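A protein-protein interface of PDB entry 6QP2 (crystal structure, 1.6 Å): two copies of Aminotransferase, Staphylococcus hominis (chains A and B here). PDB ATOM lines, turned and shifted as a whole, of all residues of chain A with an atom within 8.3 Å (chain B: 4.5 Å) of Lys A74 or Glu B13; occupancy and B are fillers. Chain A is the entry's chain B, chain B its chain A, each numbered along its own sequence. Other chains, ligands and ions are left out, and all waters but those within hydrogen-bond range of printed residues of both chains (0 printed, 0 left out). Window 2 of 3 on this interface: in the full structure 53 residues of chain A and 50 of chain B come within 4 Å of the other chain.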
ATOM      1  N   ARG A  68     -21.883 -19.134  37.293  1.00  0.00           N
ATOM      2  CA  ARG A  68     -21.995 -20.373  36.439  1.00  0.00           C
ATOM      3  C   ARG A  68     -22.695 -20.065  35.096  1.00  0.00           C
ATOM      4  O   ARG A  68     -22.240 -20.539  34.038  1.00  0.00           O
ATOM      5  CB  ARG A  68     -22.735 -21.466  37.214  1.00  0.00           C
ATOM      6  CG  ARG A  68     -21.936 -22.032  38.377  1.00  0.00           C
ATOM      7  CD  ARG A  68     -22.715 -23.015  39.219  1.00  0.00           C
ATOM      8  NE  ARG A  68     -21.916 -23.558  40.301  1.00  0.00           N
ATOM      9  CZ  ARG A  68     -22.233 -23.512  41.600  1.00  0.00           C
ATOM     10  NH1 ARG A  68     -21.404 -24.044  42.485  1.00  0.00           N
ATOM     11  NH2 ARG A  68     -23.352 -22.921  42.001  1.00  0.00           N
ATOM     12  N   GLU A  69     -23.779 -19.281  35.121  1.00  0.00           N
ATOM     13  CA  GLU A  69     -24.546 -18.947  33.918  1.00  0.00           C
ATOM     14  C   GLU A  69     -23.701 -18.061  32.991  1.00  0.00           C
ATOM     15  O   GLU A  69     -23.774 -18.173  31.768  1.00  0.00           O
ATOM     16  CB  GLU A  69     -25.867 -18.261  34.250  1.00  0.00           C
ATOM     17  CG  GLU A  69     -26.921 -19.221  34.783  1.00  0.00           C
ATOM     18  CD  GLU A  69     -28.279 -18.605  35.097  1.00  0.00           C
ATOM     19  OE1 GLU A  69     -28.486 -17.393  34.799  1.00  0.00           O
ATOM     20  OE2 GLU A  69     -29.142 -19.344  35.640  1.00  0.00           O
ATOM     21  N   ARG A  70     -22.876 -17.187  33.568  1.00  0.00           N
ATOM     22  CA  ARG A  70     -21.956 -16.379  32.729  1.00  0.00           C
ATOM     23  C   ARG A  70     -20.871 -17.272  32.108  1.00  0.00           C
ATOM     24  O   ARG A  70     -20.467 -17.061  30.958  1.00  0.00           O
ATOM     25  CB  ARG A  70     -21.359 -15.232  33.540  1.00  0.00           C
ATOM     26  CG  ARG A  70     -20.419 -14.335  32.751  1.00  0.00           C
ATOM     27  CD  ARG A  70     -21.055 -13.719  31.510  1.00  0.00           C
ATOM     28  NE  ARG A  70     -20.112 -12.904  30.744  1.00  0.00           N
ATOM     29  CZ  ARG A  70     -19.142 -13.408  29.972  1.00  0.00           C
ATOM     30  NH1 ARG A  70     -19.025 -14.716  29.855  1.00  0.00           N
ATOM     31  NH2 ARG A  70     -18.307 -12.608  29.326  1.00  0.00           N
ATOM     32  N   LEU A  71     -20.403 -18.282  32.842  1.00  0.00           N
ATOM     33  CA  LEU A  71     -19.387 -19.169  32.300  1.00  0.00           C
ATOM     34  C   LEU A  71     -19.932 -19.939  31.087  1.00  0.00           C
ATOM     35  O   LEU A  71     -19.163 -20.264  30.180  1.00  0.00           O
ATOM     36  CB  LEU A  71     -18.897 -20.135  33.372  1.00  0.00           C
ATOM     37  CG  LEU A  71     -18.099 -19.497  34.504  1.00  0.00           C
ATOM     38  CD1 LEU A  71     -17.966 -20.470  35.648  1.00  0.00           C
ATOM     39  CD2 LEU A  71     -16.738 -19.043  34.009  1.00  0.00           C
ATOM     40  N   ASN A  72     -21.235 -20.232  31.095  1.00  0.00           N
ATOM     41  CA  ASN A  72     -21.900 -20.993  30.018  1.00  0.00           C
ATOM     42  C   ASN A  72     -21.918 -20.202  28.706  1.00  0.00           C
ATOM     43  O   ASN A  72     -22.208 -20.772  27.656  1.00  0.00           O
ATOM     44  CB  ASN A  72     -23.324 -21.409  30.410  1.00  0.00           C
ATOM     45  CG  ASN A  72     -23.339 -22.490  31.468  1.00  0.00           C
ATOM     46  OD1 ASN A  72     -22.323 -23.160  31.694  1.00  0.00           O
ATOM     47  ND2 ASN A  72     -24.483 -22.678  32.106  1.00  0.00           N
ATOM     48  N   LYS A  73     -21.595 -18.912  28.774  1.00  0.00           N
ATOM     49  CA  LYS A  73     -21.488 -18.009  27.619  1.00  0.00           C
ATOM     50  C   LYS A  73     -20.108 -18.115  26.948  1.00  0.00           C
ATOM     51  O   LYS A  73     -19.873 -17.434  25.939  1.00  0.00           O
ATOM     52  CB  LYS A  73     -21.662 -16.561  28.071  1.00  0.00           C
ATOM     53  CG  LYS A  73     -22.971 -15.880  27.748  1.00  0.00           C
ATOM     54  CD  LYS A  73     -24.186 -16.549  28.230  1.00  0.00           C
ATOM     55  CE  LYS A  73     -25.307 -15.541  28.391  1.00  0.00           C
ATOM     56  NZ  LYS A  73     -26.550 -16.205  28.834  1.00  0.00           N
ATOM     57  N   LYS A  74     -19.199 -18.886  27.555  1.00  0.00           N
ATOM     58  CA  LYS A  74     -17.956 -19.446  26.960  1.00  0.00           C
ATOM     59  C   LYS A  74     -16.798 -18.442  26.808  1.00  0.00           C
ATOM     60  O   LYS A  74     -15.670 -18.858  26.775  1.00  0.00           O
ATOM     61  CB  LYS A  74     -18.243 -20.098  25.608  1.00  0.00           C
ATOM     62  CG  LYS A  74     -19.283 -21.203  25.688  1.00  0.00           C
ATOM     63  CD  LYS A  74     -19.254 -22.173  24.528  1.00  0.00           C
ATOM     64  CE  LYS A  74     -20.224 -23.307  24.758  1.00  0.00           C
ATOM     65  NZ  LYS A  74     -20.462 -24.064  23.513  1.00  0.00           N
ATOM     66  N   ILE A  75     -17.063 -17.148  26.733  1.00  0.00           N
ATOM     67  CA  ILE A  75     -16.007 -16.222  26.429  1.00  0.00           C
ATOM     68  C   ILE A  75     -15.843 -15.253  27.610  1.00  0.00           C
ATOM     69  O   ILE A  75     -16.791 -14.581  27.963  1.00  0.00           O
ATOM     70  CB  ILE A  75     -16.319 -15.496  25.106  1.00  0.00           C
ATOM     71  CG1 ILE A  75     -16.272 -16.469  23.915  1.00  0.00           C
ATOM     72  CG2 ILE A  75     -15.382 -14.342  24.915  1.00  0.00           C
ATOM     73  CD1 ILE A  75     -16.750 -15.878  22.606  1.00  0.00           C
ATOM     74  N   LEU A  76     -14.611 -15.098  28.093  1.00  0.00           N
ATOM     75  CA  LEU A  76     -14.316 -14.191  29.233  1.00  0.00           C
ATOM     76  C   LEU A  76     -13.419 -13.017  28.807  1.00  0.00           C
ATOM     77  O   LEU A  76     -12.316 -12.770  29.356  1.00  0.00           O
ATOM     78  CB  LEU A  76     -13.680 -15.042  30.331  1.00  0.00           C
ATOM     79  CG  LEU A  76     -14.579 -16.156  30.875  1.00  0.00           C
ATOM     80  CD1 LEU A  76     -13.854 -16.988  31.903  1.00  0.00           C
ATOM     81  CD2 LEU A  76     -15.841 -15.579  31.460  1.00  0.00           C
ATOM     82  N   GLY A  77     -13.890 -12.264  27.818  1.00  0.00           N
ATOM     83  CA  GLY A  77     -13.109 -11.201  27.221  1.00  0.00           C
ATOM     84  C   GLY A  77     -13.298  -9.869  27.928  1.00  0.00           C
ATOM     85  O   GLY A  77     -13.808  -9.787  29.045  1.00  0.00           O
ATOM     86  N   ASN B  10     -13.929 -27.257  18.206  1.00  0.00           N
ATOM     87  CA  ASN B  10     -14.652 -26.708  17.089  1.00  0.00           C
ATOM     88  C   ASN B  10     -14.516 -25.186  17.034  1.00  0.00           C
ATOM     89  O   ASN B  10     -15.410 -24.459  17.449  1.00  0.00           O
ATOM     90  CB  ASN B  10     -16.140 -27.035  17.129  1.00  0.00           C
ATOM     91  CG  ASN B  10     -16.854 -26.521  15.903  1.00  0.00           C
ATOM     92  OD1 ASN B  10     -16.220 -26.218  14.894  1.00  0.00           O
ATOM     93  ND2 ASN B  10     -18.167 -26.415  15.975  1.00  0.00           N
ATOM     94  N   PHE B  11     -13.464 -24.718  16.364  1.00  0.00           N
ATOM     95  CA  PHE B  11     -13.212 -23.274  16.283  1.00  0.00           C
ATOM     96  C   PHE B  11     -14.181 -22.603  15.306  1.00  0.00           C
ATOM     97  O   PHE B  11     -14.262 -21.374  15.249  1.00  0.00           O
ATOM     98  CB  PHE B  11     -11.741 -23.032  15.933  1.00  0.00           C
ATOM     99  CG  PHE B  11     -10.831 -23.468  17.045  1.00  0.00           C
ATOM    100  CD1 PHE B  11     -10.691 -22.689  18.178  1.00  0.00           C
ATOM    101  CD2 PHE B  11     -10.128 -24.659  16.969  1.00  0.00           C
ATOM    102  CE1 PHE B  11      -9.845 -23.083  19.198  1.00  0.00           C
ATOM    103  CE2 PHE B  11      -9.311 -25.066  18.006  1.00  0.00           C
ATOM    104  CZ  PHE B  11      -9.185 -24.281  19.132  1.00  0.00           C
ATOM    105  N   ASP B  12     -14.949 -23.411  14.554  1.00  0.00           N
ATOM    106  CA  ASP B  12     -15.956 -22.865  13.674  1.00  0.00           C
ATOM    107  C   ASP B  12     -17.181 -22.395  14.463  1.00  0.00           C
ATOM    108  O   ASP B  12     -17.981 -21.695  13.903  1.00  0.00           O
ATOM    109  CB  ASP B  12     -16.403 -23.864  12.611  1.00  0.00           C
ATOM    110  CG  ASP B  12     -15.268 -24.258  11.706  1.00  0.00           C
ATOM    111  OD1 ASP B  12     -14.712 -23.354  11.017  1.00  0.00           O
ATOM    112  OD2 ASP B  12     -14.890 -25.429  11.763  1.00  0.00           O
ATOM    113  N   GLU B  13     -17.328 -22.792  15.735  1.00  0.00           N
ATOM    114  CA  GLU B  13     -18.557 -22.515  16.464  1.00  0.00           C
ATOM    115  C   GLU B  13     -18.839 -21.003  16.547  1.00  0.00           C
ATOM    116  O   GLU B  13     -17.961 -20.227  16.929  1.00  0.00           O
ATOM    117  CB  GLU B  13     -18.499 -23.113  17.869  1.00  0.00           C
ATOM    118  CG  GLU B  13     -19.765 -22.848  18.652  1.00  0.00           C
ATOM    119  CD  GLU B  13     -19.811 -23.477  20.034  1.00  0.00           C
ATOM    120  OE1 GLU B  13     -18.866 -24.212  20.381  1.00  0.00           O
ATOM    121  OE2 GLU B  13     -20.806 -23.238  20.747  1.00  0.00           O
ATOM    122  N   ILE B  14     -20.095 -20.617  16.272  1.00  0.00           N
ATOM    123  CA  ILE B  14     -20.563 -19.232  16.403  1.00  0.00           C
ATOM    124  C   ILE B  14     -21.074 -19.073  17.832  1.00  0.00           C
ATOM    125  O   ILE B  14     -22.045 -19.731  18.214  1.00  0.00           O
ATOM    126  CB  ILE B  14     -21.660 -18.916  15.358  1.00  0.00           C
ATOM    127  CG1 ILE B  14     -21.194 -19.208  13.927  1.00  0.00           C
ATOM    128  CG2 ILE B  14     -22.197 -17.495  15.506  1.00  0.00           C
ATOM    129  CD1 ILE B  14     -19.842 -18.623  13.569  1.00  0.00           C
ATOM    130  N   ILE B  15     -20.399 -18.246  18.627  1.00  0.00           N
ATOM    131  CA  ILE B  15     -20.716 -18.082  20.012  1.00  0.00           C
ATOM    132  C   ILE B  15     -21.339 -16.703  20.194  1.00  0.00           C
ATOM    133  O   ILE B  15     -20.736 -15.678  19.844  1.00  0.00           O
ATOM    134  CB  ILE B  15     -19.487 -18.260  20.917  1.00  0.00           C
ATOM    135  CG1 ILE B  15     -18.920 -19.675  20.858  1.00  0.00           C
ATOM    136  CG2 ILE B  15     -19.813 -17.850  22.339  1.00  0.00           C
ATOM    137  CD1 ILE B  15     -17.495 -19.761  21.342  1.00  0.00           C
ATOM    138  N   GLY B  58     -14.193 -19.861  21.933  1.00  0.00           N
ATOM    139  CA  GLY B  58     -14.509 -20.133  23.299  1.00  0.00           C
ATOM    140  C   GLY B  58     -13.253 -20.217  24.136  1.00  0.00           C
ATOM    141  O   GLY B  58     -12.280 -20.828  23.728  1.00  0.00           O
ATOM    142  N   THR B  59     -13.273 -19.597  25.316  1.00  0.00           N
ATOM    143  CA  THR B  59     -12.341 -19.932  26.344  1.00  0.00           C
ATOM    144  C   THR B  59     -12.450 -21.434  26.541  1.00  0.00           C
ATOM    145  O   THR B  59     -13.556 -21.942  26.673  1.00  0.00           O
ATOM    146  CB  THR B  59     -12.661 -19.228  27.673  1.00  0.00           C
ATOM    147  OG1 THR B  59     -12.708 -17.812  27.495  1.00  0.00           O
ATOM    148  CG2 THR B  59     -11.656 -19.601  28.741  1.00  0.00           C
ATOM    149  N   GLU B  61     -12.836 -25.291  27.639  1.00  0.00           N
ATOM    150  CA  GLU B  61     -13.535 -25.912  28.744  1.00  0.00           C
ATOM    151  C   GLU B  61     -12.578 -26.313  29.875  1.00  0.00           C
ATOM    152  O   GLU B  61     -13.034 -26.328  31.002  1.00  0.00           O
ATOM    153  CB  GLU B  61     -14.389 -27.081  28.234  1.00  0.00           C
ATOM    154  CG  GLU B  61     -15.595 -26.645  27.405  1.00  0.00           C
ATOM    155  CD  GLU B  61     -16.655 -25.783  28.089  1.00  0.00           C
ATOM    156  OE1 GLU B  61     -16.881 -25.950  29.340  1.00  0.00           O
ATOM    157  OE2 GLU B  61     -17.265 -24.919  27.378  1.00  0.00           O
ATOM    158  N   LEU B  64     -12.627 -23.172  31.878  1.00  0.00           N
ATOM    159  CA  LEU B  64     -13.920 -22.880  32.453  1.00  0.00           C
ATOM    160  C   LEU B  64     -14.260 -23.888  33.574  1.00  0.00           C
ATOM    161  O   LEU B  64     -14.886 -23.533  34.563  1.00  0.00           O
ATOM    162  CB  LEU B  64     -14.997 -22.887  31.377  1.00  0.00           C
ATOM    163  CG  LEU B  64     -14.829 -21.859  30.260  1.00  0.00           C
ATOM    164  CD1 LEU B  64     -15.943 -22.005  29.247  1.00  0.00           C
ATOM    165  CD2 LEU B  64     -14.795 -20.456  30.840  1.00  0.00           C
ATOM    166  N   PRO B 388     -14.300 -17.444  13.765  1.00  0.00           N
ATOM    167  CA  PRO B 388     -14.595 -18.537  12.843  1.00  0.00           C
ATOM    168  C   PRO B 388     -14.236 -18.117  11.418  1.00  0.00           C
ATOM    169  O   PRO B 388     -14.498 -16.987  11.003  1.00  0.00           O
ATOM    170  CB  PRO B 388     -16.103 -18.765  13.046  1.00  0.00           C
ATOM    171  CG  PRO B 388     -16.274 -18.444  14.499  1.00  0.00           C
ATOM    172  CD  PRO B 388     -15.449 -17.181  14.652  1.00  0.00           C
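Glu B13 touches one residue of chain A. Printed residues of chain B within 4 Å of Ile A75: Ile B15 and Thr B59. Printed residues of chain A within 4 Å of Gly B58: Lys A74 (3.8 Å). Asp B12 touches none of the printed residues of chain A. The nearest printed residue of chain B that does not touch Lys A74 is Ile B15 (4.3 Å). The nearest residue of chain A that does not touch Glu B13 is Ile A75 (7.3 Å). The nearest printed residue of chain B that does not touch Leu A76 is Gly B58 (6.6 Å).
No position is printed for both chains. Of the 10 pairs that touch across the chains among the printed residues, none has its exchanged pair printed and touching as well.
Leu B64 touches Leu A71. Lys A73 touches Ile B15. Lys A74 touches Gly B58. Lys A74 touches Leu B64 (CA to CD1, 3.98 Å). Ile B15 touches Ile A75 (CG2 to CD1, 3.7 Å). Ile A75 touches Thr B59. Leu A76 touches Leu B64.
The backbone carbonyl oxygen of Ile A75 is in hydrogen-bond range of the guanidinium group of Arg A70, 2.8 Å away.
Of the 10 printed residues of chain A, 5 touch a printed residue of chain B. Hydrophobic or aromatic side chains of chain A within 4 Å of the printed part of chain B: Leu A71, Ile A75 and Leu A76. Hydrophobic or aromatic side chains of chain B within 4 Å of the printed part of chain A: Ile B15 and Leu B64. Among the printed residues, Asp or Glu carboxylates within 4 Å of a Lys or Arg side-chain nitrogen of the other chain: Lys A74 with Glu B13 (2.9 Å).
The side-chain hydroxyl (OG1) of Thr B59 is in hydrogen-bond range of the backbone NH (N) of Leu A76, 3.4 Å away. The backbone NH (N) of Thr B59 is in hydrogen-bond range of the backbone carbonyl oxygen (O) of Lys A74, at 2.9 Å. The side-chain carboxylate (OE2) of Glu B13 is in salt-bridge range of the side-chain amino group (NZ) of Lys A74.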
